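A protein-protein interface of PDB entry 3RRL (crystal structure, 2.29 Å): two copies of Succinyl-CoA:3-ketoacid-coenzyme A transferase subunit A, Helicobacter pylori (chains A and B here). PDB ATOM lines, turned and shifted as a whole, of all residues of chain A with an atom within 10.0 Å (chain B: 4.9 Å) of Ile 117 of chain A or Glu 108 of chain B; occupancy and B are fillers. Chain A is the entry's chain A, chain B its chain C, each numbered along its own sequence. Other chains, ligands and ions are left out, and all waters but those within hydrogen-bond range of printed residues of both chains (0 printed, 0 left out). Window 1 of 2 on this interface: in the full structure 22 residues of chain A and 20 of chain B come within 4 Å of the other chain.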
ATOM      1  N   ALA A 107     -10.056  -7.556 -21.693  1.00  0.00           N
ATOM      2  CA  ALA A 107      -8.903  -6.676 -21.843  1.00  0.00           C
ATOM      3  C   ALA A 107      -9.334  -5.285 -22.305  1.00  0.00           C
ATOM      4  O   ALA A 107      -8.935  -4.275 -21.714  1.00  0.00           O
ATOM      5  CB  ALA A 107      -7.905  -7.264 -22.811  1.00  0.00           C
ATOM      6  N   GLU A 108     -10.151  -5.232 -23.355  1.00  0.00           N
ATOM      7  CA  GLU A 108     -10.526  -3.952 -23.936  1.00  0.00           C
ATOM      8  C   GLU A 108     -11.461  -3.177 -23.023  1.00  0.00           C
ATOM      9  O   GLU A 108     -11.369  -1.951 -22.940  1.00  0.00           O
ATOM     10  CB  GLU A 108     -11.152  -4.113 -25.319  1.00  0.00           C
ATOM     11  CG  GLU A 108     -11.273  -2.798 -26.056  1.00  0.00           C
ATOM     12  CD  GLU A 108      -9.917  -2.128 -26.277  1.00  0.00           C
ATOM     13  OE1 GLU A 108      -8.906  -2.843 -26.472  1.00  0.00           O
ATOM     14  OE2 GLU A 108      -9.861  -0.881 -26.252  1.00  0.00           O
ATOM     15  N   ASN A 109     -12.358  -3.881 -22.336  1.00  0.00           N
ATOM     16  CA  ASN A 109     -13.194  -3.225 -21.334  1.00  0.00           C
ATOM     17  C   ASN A 109     -12.346  -2.500 -20.296  1.00  0.00           C
ATOM     18  O   ASN A 109     -12.693  -1.407 -19.845  1.00  0.00           O
ATOM     19  CB  ASN A 109     -14.113  -4.230 -20.645  1.00  0.00           C
ATOM     20  CG  ASN A 109     -15.235  -4.702 -21.541  1.00  0.00           C
ATOM     21  OD1 ASN A 109     -15.278  -4.372 -22.729  1.00  0.00           O
ATOM     22  ND2 ASN A 109     -16.143  -5.495 -20.981  1.00  0.00           N
ATOM     23  N   LEU A 110     -11.230  -3.115 -19.919  1.00  0.00           N
ATOM     24  CA  LEU A 110     -10.319  -2.519 -18.946  1.00  0.00           C
ATOM     25  C   LEU A 110      -9.624  -1.331 -19.571  1.00  0.00           C
ATOM     26  O   LEU A 110      -9.517  -0.254 -18.955  1.00  0.00           O
ATOM     27  CB  LEU A 110      -9.287  -3.540 -18.469  1.00  0.00           C
ATOM     28  CG  LEU A 110      -9.907  -4.595 -17.556  1.00  0.00           C
ATOM     29  CD1 LEU A 110      -8.990  -5.808 -17.365  1.00  0.00           C
ATOM     30  CD2 LEU A 110     -10.267  -3.965 -16.221  1.00  0.00           C
ATOM     31  N   HIS A 111      -9.154  -1.524 -20.799  1.00  0.00           N
ATOM     32  CA  HIS A 111      -8.539  -0.429 -21.530  1.00  0.00           C
ATOM     33  C   HIS A 111      -9.513   0.753 -21.585  1.00  0.00           C
ATOM     34  O   HIS A 111      -9.159   1.883 -21.227  1.00  0.00           O
ATOM     35  CB  HIS A 111      -8.136  -0.876 -22.933  1.00  0.00           C
ATOM     36  CG  HIS A 111      -7.455   0.190 -23.730  1.00  0.00           C
ATOM     37  ND1 HIS A 111      -8.131   1.009 -24.611  1.00  0.00           N
ATOM     38  CD2 HIS A 111      -6.159   0.585 -23.768  1.00  0.00           C
ATOM     39  CE1 HIS A 111      -7.281   1.856 -25.163  1.00  0.00           C
ATOM     40  NE2 HIS A 111      -6.079   1.619 -24.668  1.00  0.00           N
ATOM     41  N   ALA A 112     -10.751   0.490 -22.003  1.00  0.00           N
ATOM     42  CA  ALA A 112     -11.757   1.552 -22.089  1.00  0.00           C
ATOM     43  C   ALA A 112     -11.930   2.278 -20.748  1.00  0.00           C
ATOM     44  O   ALA A 112     -11.996   3.506 -20.696  1.00  0.00           O
ATOM     45  CB  ALA A 112     -13.081   0.995 -22.577  1.00  0.00           C
ATOM     46  N   GLY A 113     -11.985   1.510 -19.665  1.00  0.00           N
ATOM     47  CA  GLY A 113     -12.135   2.067 -18.333  1.00  0.00           C
ATOM     48  C   GLY A 113     -11.001   2.987 -17.918  1.00  0.00           C
ATOM     49  O   GLY A 113     -11.221   4.005 -17.268  1.00  0.00           O
ATOM     50  N   GLY A 114      -9.777   2.633 -18.288  1.00  0.00           N
ATOM     51  CA  GLY A 114      -8.636   3.476 -17.982  1.00  0.00           C
ATOM     52  C   GLY A 114      -8.556   4.670 -18.921  1.00  0.00           C
ATOM     53  O   GLY A 114      -8.004   5.715 -18.570  1.00  0.00           O
ATOM     54  N   ALA A 115      -9.113   4.519 -20.122  1.00  0.00           N
ATOM     55  CA  ALA A 115      -8.980   5.545 -21.149  1.00  0.00           C
ATOM     56  C   ALA A 115     -10.164   6.523 -21.247  1.00  0.00           C
ATOM     57  O   ALA A 115     -10.170   7.414 -22.100  1.00  0.00           O
ATOM     58  CB  ALA A 115      -8.695   4.902 -22.494  1.00  0.00           C
ATOM     59  N   GLY A 116     -11.156   6.356 -20.376  1.00  0.00           N
ATOM     60  CA  GLY A 116     -12.285   7.276 -20.317  1.00  0.00           C
ATOM     61  C   GLY A 116     -13.319   7.030 -21.399  1.00  0.00           C
ATOM     62  O   GLY A 116     -14.099   7.910 -21.748  1.00  0.00           O
ATOM     63  N   ILE A 117     -13.308   5.818 -21.942  1.00  0.00           N
ATOM     64  CA  ILE A 117     -14.289   5.400 -22.922  1.00  0.00           C
ATOM     65  C   ILE A 117     -15.334   4.517 -22.238  1.00  0.00           C
ATOM     66  O   ILE A 117     -15.024   3.422 -21.796  1.00  0.00           O
ATOM     67  CB  ILE A 117     -13.607   4.619 -24.046  1.00  0.00           C
ATOM     68  CG1 ILE A 117     -12.561   5.502 -24.734  1.00  0.00           C
ATOM     69  CG2 ILE A 117     -14.642   4.074 -25.034  1.00  0.00           C
ATOM     70  CD1 ILE A 117     -11.580   4.717 -25.576  1.00  0.00           C
ATOM     71  N   PRO A 118     -16.577   5.007 -22.137  1.00  0.00           N
ATOM     72  CA  PRO A 118     -17.658   4.315 -21.425  1.00  0.00           C
ATOM     73  C   PRO A 118     -18.112   3.035 -22.123  1.00  0.00           C
ATOM     74  O   PRO A 118     -18.493   2.066 -21.462  1.00  0.00           O
ATOM     75  CB  PRO A 118     -18.791   5.348 -21.434  1.00  0.00           C
ATOM     76  CG  PRO A 118     -18.545   6.151 -22.670  1.00  0.00           C
ATOM     77  CD  PRO A 118     -17.045   6.256 -22.769  1.00  0.00           C
ATOM     78  N   ALA A 119     -18.089   3.038 -23.451  1.00  0.00           N
ATOM     79  CA  ALA A 119     -18.549   1.888 -24.216  1.00  0.00           C
ATOM     80  C   ALA A 119     -17.972   1.912 -25.624  1.00  0.00           C
ATOM     81  O   ALA A 119     -17.590   2.969 -26.122  1.00  0.00           O
ATOM     82  CB  ALA A 119     -20.079   1.879 -24.269  1.00  0.00           C
ATOM     83  N   TYR A 120     -17.933   0.746 -26.265  1.00  0.00           N
ATOM     84  CA  TYR A 120     -17.423   0.608 -27.626  1.00  0.00           C
ATOM     85  C   TYR A 120     -18.057  -0.634 -28.233  1.00  0.00           C
ATOM     86  O   TYR A 120     -18.620  -1.458 -27.520  1.00  0.00           O
ATOM     87  CB  TYR A 120     -15.900   0.454 -27.628  1.00  0.00           C
ATOM     88  CG  TYR A 120     -15.456  -0.824 -26.966  1.00  0.00           C
ATOM     89  CD1 TYR A 120     -15.181  -1.960 -27.725  1.00  0.00           C
ATOM     90  CD2 TYR A 120     -15.342  -0.912 -25.581  1.00  0.00           C
ATOM     91  CE1 TYR A 120     -14.795  -3.150 -27.128  1.00  0.00           C
ATOM     92  CE2 TYR A 120     -14.957  -2.099 -24.974  1.00  0.00           C
ATOM     93  CZ  TYR A 120     -14.694  -3.216 -25.757  1.00  0.00           C
ATOM     94  OH  TYR A 120     -14.308  -4.401 -25.173  1.00  0.00           O
ATOM     95  N   TYR A 121     -17.964  -0.769 -29.549  1.00  0.00           N
ATOM     96  CA  TYR A 121     -18.543  -1.924 -30.224  1.00  0.00           C
ATOM     97  C   TYR A 121     -17.512  -2.971 -30.609  1.00  0.00           C
ATOM     98  O   TYR A 121     -16.399  -2.651 -31.025  1.00  0.00           O
ATOM     99  CB  TYR A 121     -19.319  -1.481 -31.451  1.00  0.00           C
ATOM    100  CG  TYR A 121     -20.594  -0.760 -31.105  1.00  0.00           C
ATOM    101  CD1 TYR A 121     -21.733  -1.466 -30.754  1.00  0.00           C
ATOM    102  CD2 TYR A 121     -20.660   0.626 -31.125  1.00  0.00           C
ATOM    103  CE1 TYR A 121     -22.902  -0.814 -30.431  1.00  0.00           C
ATOM    104  CE2 TYR A 121     -21.831   1.289 -30.805  1.00  0.00           C
ATOM    105  CZ  TYR A 121     -22.947   0.564 -30.458  1.00  0.00           C
ATOM    106  OH  TYR A 121     -24.119   1.213 -30.137  1.00  0.00           O
ATOM    107  N   LEU A 146     -22.507  -3.925 -28.158  1.00  0.00           N
ATOM    108  CA  LEU A 146     -22.000  -2.868 -27.301  1.00  0.00           C
ATOM    109  C   LEU A 146     -21.374  -3.445 -26.031  1.00  0.00           C
ATOM    110  O   LEU A 146     -22.022  -4.195 -25.283  1.00  0.00           O
ATOM    111  CB  LEU A 146     -23.145  -1.923 -26.934  1.00  0.00           C
ATOM    112  CG  LEU A 146     -22.776  -0.620 -26.230  1.00  0.00           C
ATOM    113  CD1 LEU A 146     -21.828   0.176 -27.104  1.00  0.00           C
ATOM    114  CD2 LEU A 146     -24.031   0.181 -25.924  1.00  0.00           C
ATOM    115  N   GLU A 147     -20.110  -3.109 -25.790  1.00  0.00           N
ATOM    116  CA  GLU A 147     -19.452  -3.503 -24.543  1.00  0.00           C
ATOM    117  C   GLU A 147     -19.128  -2.287 -23.692  1.00  0.00           C
ATOM    118  O   GLU A 147     -18.764  -1.226 -24.210  1.00  0.00           O
ATOM    119  CB  GLU A 147     -18.174  -4.291 -24.817  1.00  0.00           C
ATOM    120  CG  GLU A 147     -18.412  -5.713 -25.274  1.00  0.00           C
ATOM    121  CD  GLU A 147     -18.999  -6.591 -24.180  1.00  0.00           C
ATOM    122  OE1 GLU A 147     -18.999  -6.169 -23.002  1.00  0.00           O
ATOM    123  OE2 GLU A 147     -19.462  -7.706 -24.504  1.00  0.00           O
ATOM    124  N   ARG A 148     -19.253  -2.452 -22.383  1.00  0.00           N
ATOM    125  CA  ARG A 148     -19.052  -1.361 -21.452  1.00  0.00           C
ATOM    126  C   ARG A 148     -17.734  -1.464 -20.705  1.00  0.00           C
ATOM    127  O   ARG A 148     -17.227  -2.556 -20.448  1.00  0.00           O
ATOM    128  CB  ARG A 148     -20.227  -1.278 -20.483  1.00  0.00           C
ATOM    129  CG  ARG A 148     -21.440  -0.603 -21.120  1.00  0.00           C
ATOM    130  CD  ARG A 148     -22.736  -1.078 -20.516  1.00  0.00           C
ATOM    131  NE  ARG A 148     -23.715   0.006 -20.436  1.00  0.00           N
ATOM    132  CZ  ARG A 148     -24.612   0.285 -21.375  1.00  0.00           C
ATOM    133  NH1 ARG A 148     -25.459   1.291 -21.201  1.00  0.00           N
ATOM    134  NH2 ARG A 148     -24.667  -0.437 -22.486  1.00  0.00           N
ATOM    135  N   ALA A 149     -17.186  -0.303 -20.376  1.00  0.00           N
ATOM    136  CA  ALA A 149     -15.918  -0.209 -19.678  1.00  0.00           C
ATOM    137  C   ALA A 149     -15.994  -0.834 -18.291  1.00  0.00           C
ATOM    138  O   ALA A 149     -17.061  -0.908 -17.674  1.00  0.00           O
ATOM    139  CB  ALA A 149     -15.481   1.254 -19.576  1.00  0.00           C
ATOM    140  N   ILE A 150     -14.840  -1.287 -17.820  1.00  0.00           N
ATOM    141  CA  ILE A 150     -14.693  -1.814 -16.479  1.00  0.00           C
ATOM    142  C   ILE A 150     -13.734  -0.928 -15.695  1.00  0.00           C
ATOM    143  O   ILE A 150     -12.664  -0.563 -16.193  1.00  0.00           O
ATOM    144  CB  ILE A 150     -14.124  -3.241 -16.518  1.00  0.00           C
ATOM    145  CG1 ILE A 150     -15.200  -4.239 -16.961  1.00  0.00           C
ATOM    146  CG2 ILE A 150     -13.549  -3.626 -15.160  1.00  0.00           C
ATOM    147  CD1 ILE A 150     -14.633  -5.631 -17.283  1.00  0.00           C
ATOM    148  N   THR A 151     -14.127  -0.573 -14.475  1.00  0.00           N
ATOM    149  CA  THR A 151     -13.258   0.172 -13.579  1.00  0.00           C
ATOM    150  C   THR A 151     -13.332  -0.481 -12.210  1.00  0.00           C
ATOM    151  O   THR A 151     -14.232  -1.267 -11.940  1.00  0.00           O
ATOM    152  CB  THR A 151     -13.659   1.666 -13.461  1.00  0.00           C
ATOM    153  OG1 THR A 151     -15.029   1.768 -13.057  1.00  0.00           O
ATOM    154  CG2 THR A 151     -13.475   2.394 -14.791  1.00  0.00           C
ATOM    155  N   MET A 183      -4.435   1.039 -14.987  1.00  0.00           N
ATOM    156  CA  MET A 183      -5.056   2.257 -15.502  1.00  0.00           C
ATOM    157  C   MET A 183      -6.547   2.353 -15.172  1.00  0.00           C
ATOM    158  O   MET A 183      -7.073   3.447 -14.993  1.00  0.00           O
ATOM    159  CB  MET A 183      -4.822   2.380 -17.008  1.00  0.00           C
ATOM    160  CG  MET A 183      -3.355   2.361 -17.387  1.00  0.00           C
ATOM    161  SD  MET A 183      -3.078   2.433 -19.315  1.00  0.00           S
ATOM    162  CE  MET A 183      -3.498   0.615 -19.771  1.00  0.00           C
ATOM    163  N   ALA A 184      -7.219   1.209 -15.075  1.00  0.00           N
ATOM    164  CA  ALA A 184      -8.669   1.187 -14.846  1.00  0.00           C
ATOM    165  C   ALA A 184      -9.075   1.305 -13.367  1.00  0.00           C
ATOM    166  O   ALA A 184     -10.258   1.385 -13.048  1.00  0.00           O
ATOM    167  CB  ALA A 184      -9.290  -0.074 -15.472  1.00  0.00           C
ATOM    168  N   GLY B 104      -7.225  13.675 -29.598  1.00  0.00           N
ATOM    169  CA  GLY B 104      -7.507  12.442 -28.889  1.00  0.00           C
ATOM    170  C   GLY B 104      -8.433  11.519 -29.665  1.00  0.00           C
ATOM    171  O   GLY B 104      -8.280  10.291 -29.645  1.00  0.00           O
ATOM    172  N   THR B 105      -9.404  12.112 -30.347  1.00  0.00           N
ATOM    173  CA  THR B 105     -10.319  11.350 -31.186  1.00  0.00           C
ATOM    174  C   THR B 105      -9.593  10.788 -32.404  1.00  0.00           C
ATOM    175  O   THR B 105      -9.777   9.631 -32.767  1.00  0.00           O
ATOM    176  CB  THR B 105     -11.501  12.217 -31.648  1.00  0.00           C
ATOM    177  OG1 THR B 105     -12.282  12.584 -30.507  1.00  0.00           O
ATOM    178  CG2 THR B 105     -12.385  11.451 -32.641  1.00  0.00           C
ATOM    179  N   LEU B 106      -8.765  11.614 -33.032  1.00  0.00           N
ATOM    180  CA  LEU B 106      -7.959  11.165 -34.155  1.00  0.00           C
ATOM    181  C   LEU B 106      -7.133   9.952 -33.726  1.00  0.00           C
ATOM    182  O   LEU B 106      -7.192   8.896 -34.363  1.00  0.00           O
ATOM    183  CB  LEU B 106      -7.047  12.290 -34.641  1.00  0.00           C
ATOM    184  CG  LEU B 106      -6.291  12.084 -35.959  1.00  0.00           C
ATOM    185  CD1 LEU B 106      -7.256  11.887 -37.113  1.00  0.00           C
ATOM    186  CD2 LEU B 106      -5.370  13.270 -36.235  1.00  0.00           C
ATOM    187  N   ALA B 107      -6.376  10.091 -32.638  1.00  0.00           N
ATOM    188  CA  ALA B 107      -5.563   8.972 -32.170  1.00  0.00           C
ATOM    189  C   ALA B 107      -6.408   7.716 -31.889  1.00  0.00           C
ATOM    190  O   ALA B 107      -6.019   6.598 -32.236  1.00  0.00           O
ATOM    191  CB  ALA B 107      -4.733   9.364 -30.931  1.00  0.00           C
ATOM    192  N   GLU B 108      -7.564   7.896 -31.264  1.00  0.00           N
ATOM    193  CA  GLU B 108      -8.343   6.740 -30.844  1.00  0.00           C
ATOM    194  C   GLU B 108      -9.084   6.115 -32.035  1.00  0.00           C
ATOM    195  O   GLU B 108      -9.264   4.897 -32.093  1.00  0.00           O
ATOM    196  CB  GLU B 108      -9.288   7.097 -29.690  1.00  0.00           C
ATOM    197  CG  GLU B 108      -9.894   5.888 -28.978  1.00  0.00           C
ATOM    198  CD  GLU B 108      -8.844   4.923 -28.410  1.00  0.00           C
ATOM    199  OE1 GLU B 108      -7.782   5.387 -27.951  1.00  0.00           O
ATOM    200  OE2 GLU B 108      -9.087   3.694 -28.415  1.00  0.00           O
ATOM    201  N   ASN B 109      -9.488   6.950 -32.989  1.00  0.00           N
ATOM    202  CA  ASN B 109     -10.047   6.462 -34.247  1.00  0.00           C
ATOM    203  C   ASN B 109      -9.086   5.519 -34.969  1.00  0.00           C
ATOM    204  O   ASN B 109      -9.496   4.481 -35.496  1.00  0.00           O
ATOM    205  CB  ASN B 109     -10.405   7.627 -35.179  1.00  0.00           C
ATOM    206  CG  ASN B 109     -11.647   8.379 -34.730  1.00  0.00           C
ATOM    207  OD1 ASN B 109     -12.317   7.973 -33.779  1.00  0.00           O
ATOM    208  ND2 ASN B 109     -11.970   9.472 -35.423  1.00  0.00           N
ATOM    209  N   LEU B 110      -7.809   5.894 -34.994  1.00  0.00           N
ATOM    210  CA  LEU B 110      -6.789   5.104 -35.669  1.00  0.00           C
ATOM    211  C   LEU B 110      -6.564   3.827 -34.907  1.00  0.00           C
ATOM    212  O   LEU B 110      -6.490   2.746 -35.491  1.00  0.00           O
ATOM    213  CB  LEU B 110      -5.474   5.883 -35.776  1.00  0.00           C
ATOM    214  CG  LEU B 110      -5.484   7.069 -36.754  1.00  0.00           C
ATOM    215  CD1 LEU B 110      -4.244   7.971 -36.583  1.00  0.00           C
ATOM    216  CD2 LEU B 110      -5.610   6.567 -38.197  1.00  0.00           C
ATOM    217  N   HIS B 111      -6.446   3.961 -33.589  1.00  0.00           N
ATOM    218  CA  HIS B 111      -6.285   2.807 -32.736  1.00  0.00           C
ATOM    219  C   HIS B 111      -7.432   1.830 -32.925  1.00  0.00           C
ATOM    220  O   HIS B 111      -7.210   0.625 -33.039  1.00  0.00           O
ATOM    221  CB  HIS B 111      -6.189   3.215 -31.269  1.00  0.00           C
ATOM    222  CG  HIS B 111      -5.936   2.062 -30.353  1.00  0.00           C
ATOM    223  ND1 HIS B 111      -6.941   1.444 -29.642  1.00  0.00           N
ATOM    224  CD2 HIS B 111      -4.798   1.389 -30.063  1.00  0.00           C
ATOM    225  CE1 HIS B 111      -6.429   0.452 -28.935  1.00  0.00           C
ATOM    226  NE2 HIS B 111      -5.131   0.397 -29.173  1.00  0.00           N
ATOM    227  N   ALA B 112      -8.658   2.346 -32.955  1.00  0.00           N
ATOM    228  CA  ALA B 112      -9.829   1.495 -33.163  1.00  0.00           C
ATOM    229  C   ALA B 112      -9.745   0.785 -34.517  1.00  0.00           C
ATOM    230  O   ALA B 112     -10.018  -0.422 -34.627  1.00  0.00           O
ATOM    231  CB  ALA B 112     -11.094   2.304 -33.053  1.00  0.00           C
ATOM    232  N   GLY B 113      -9.327   1.531 -35.539  1.00  0.00           N
ATOM    233  CA  GLY B 113      -9.138   0.970 -36.866  1.00  0.00           C
ATOM    234  C   GLY B 113      -8.174  -0.201 -36.883  1.00  0.00           C
ATOM    235  O   GLY B 113      -8.422  -1.206 -37.549  1.00  0.00           O
ATOM    236  N   TYR B 120     -16.819   3.816 -31.012  1.00  0.00           N
ATOM    237  CA  TYR B 120     -16.656   3.926 -29.571  1.00  0.00           C
ATOM    238  C   TYR B 120     -17.170   5.304 -29.172  1.00  0.00           C
ATOM    239  O   TYR B 120     -17.304   6.185 -30.023  1.00  0.00           O
ATOM    240  CB  TYR B 120     -15.174   3.777 -29.191  1.00  0.00           C
ATOM    241  CG  TYR B 120     -14.328   4.920 -29.706  1.00  0.00           C
ATOM    242  CD1 TYR B 120     -14.125   6.054 -28.932  1.00  0.00           C
ATOM    243  CD2 TYR B 120     -13.753   4.879 -30.979  1.00  0.00           C
ATOM    244  CE1 TYR B 120     -13.373   7.116 -29.399  1.00  0.00           C
ATOM    245  CE2 TYR B 120     -12.996   5.941 -31.458  1.00  0.00           C
ATOM    246  CZ  TYR B 120     -12.816   7.060 -30.660  1.00  0.00           C
ATOM    247  OH  TYR B 120     -12.075   8.131 -31.109  1.00  0.00           O
ATOM    248  N   TYR B 121     -17.458   5.501 -27.889  1.00  0.00           N
ATOM    249  CA  TYR B 121     -17.953   6.791 -27.416  1.00  0.00           C
ATOM    250  C   TYR B 121     -16.867   7.577 -26.735  1.00  0.00           C
ATOM    251  O   TYR B 121     -15.992   7.003 -26.086  1.00  0.00           O
ATOM    252  CB  TYR B 121     -19.122   6.620 -26.449  1.00  0.00           C
ATOM    253  CG  TYR B 121     -20.368   6.082 -27.113  1.00  0.00           C
ATOM    254  CD1 TYR B 121     -21.312   6.942 -27.669  1.00  0.00           C
ATOM    255  CD2 TYR B 121     -20.594   4.715 -27.197  1.00  0.00           C
ATOM    256  CE1 TYR B 121     -22.456   6.445 -28.288  1.00  0.00           C
ATOM    257  CE2 TYR B 121     -21.734   4.212 -27.811  1.00  0.00           C
ATOM    258  CZ  TYR B 121     -22.657   5.080 -28.352  1.00  0.00           C
ATOM    259  OH  TYR B 121     -23.779   4.575 -28.953  1.00  0.00           O
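Leu 110 of chain A touches none of the printed residues of chain B.
Ile 117 of chain A touches just these residues of chain B: Glu 108 and Tyr 121.
Printed residues of chain B within 4 Å of Tyr 120 of chain A: Tyr 120 (3.7 Å).
Of chain A, only Ile 117 (3.9 Å) comes within 4 Å of Glu 108 of chain B.
His 111 of chain B touches none of the printed residues of chain A.
No residue of chain A comes within 4 Å of Ala 112 of chain B.
Of the printed residues of chain A, Tyr 120 of chain B touches Ala 119 and Tyr 120.
Of the printed residues of chain A, Tyr 121 of chain B touches Ile 117, Pro 118, Ala 119 and Tyr 121.
The nearest residue of chain B that does not touch Ile 117 of chain A is Tyr 120 of chain B (4.2 Å).
The nearest residue of chain A that does not touch Glu 108 of chain B is His 111 of chain A (4.1 Å).
Hydrophobic or aromatic side chains of chain A that line the printed part of chain B: Ile 117, Pro 118, Tyr 120 and Tyr 121.
Of the 12 printed residues of chain B, 3 touch a printed residue of chain A.
Printed residues of chain B that touch a printed residue of chain A: Glu 108, Tyr 120 and Tyr 121.
Hydrophobic or aromatic side chains of chain B that line the printed part of chain A: Tyr 120 and Tyr 121.
Among the printed residues, 7 pairs touch across the chains.
Among the printed residues, no Asp or Glu carboxylate lies within 4 Å of a Lys or Arg side-chain nitrogen of the other chain.
The backbone carbonyl oxygen (O) of Ala 119 of chain A sits at hydrogen-bond distance from the backbone NH (N) of Tyr 121 of chain B (3.1 Å).
OH of Tyr 120 of chain A is in hydrogen-bond range of OD1 of Asn 109 of chain A, at 2.6 Å.
The backbone carbonyl oxygen of Thr 105 of chain B lies within hydrogen-bond range of the side-chain hydroxyl of Tyr 120 of chain B, at 3.2 Å.
The backbone NH (N) of Ala 149 of chain A is in hydrogen-bond range of the backbone carbonyl oxygen (O) of Pro 118 of chain A (2.9 Å).
OD1 of Asn 109 of chain B is in hydrogen-bond range of OH of Tyr 120 of chain B, at 2.7 Å.
The backbone NH (N) of Glu 147 of chain A sits at hydrogen-bond distance from the backbone carbonyl oxygen (O) of Tyr 120 of chain A, at 2.8 Å.
O of Ala 112 of chain A lies within hydrogen-bond range of N of Ile 117 of chain A, at 2.9 Å.
Tyr 120 of chain A touches its own counterpart, Tyr 120 of chain B.
Tyr 121 of chain B touches its own counterpart, Tyr 121 of chain A.
9 positions are printed for both chains.
Of the 7 pairs that touch across the chains among the printed residues, 2 have their exchanged pair printed and touching as well.
Among the printed residues, pairs that only touch across the chains: Ile 117 of chain A with Glu 108 of chain B (3.9 Å), Ile 117 of chain A with Tyr 121 of chain B (3.4 Å), Pro 118 of chain A with Tyr 121 of chain B (3.6 Å), Ala 119 of chain A with Tyr 120 of chain B (3.7 Å), Tyr 120 of chain A with Tyr 120 of chain B (3.7 Å) and Tyr 121 of chain A with Tyr 121 of chain B (3.6 Å).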
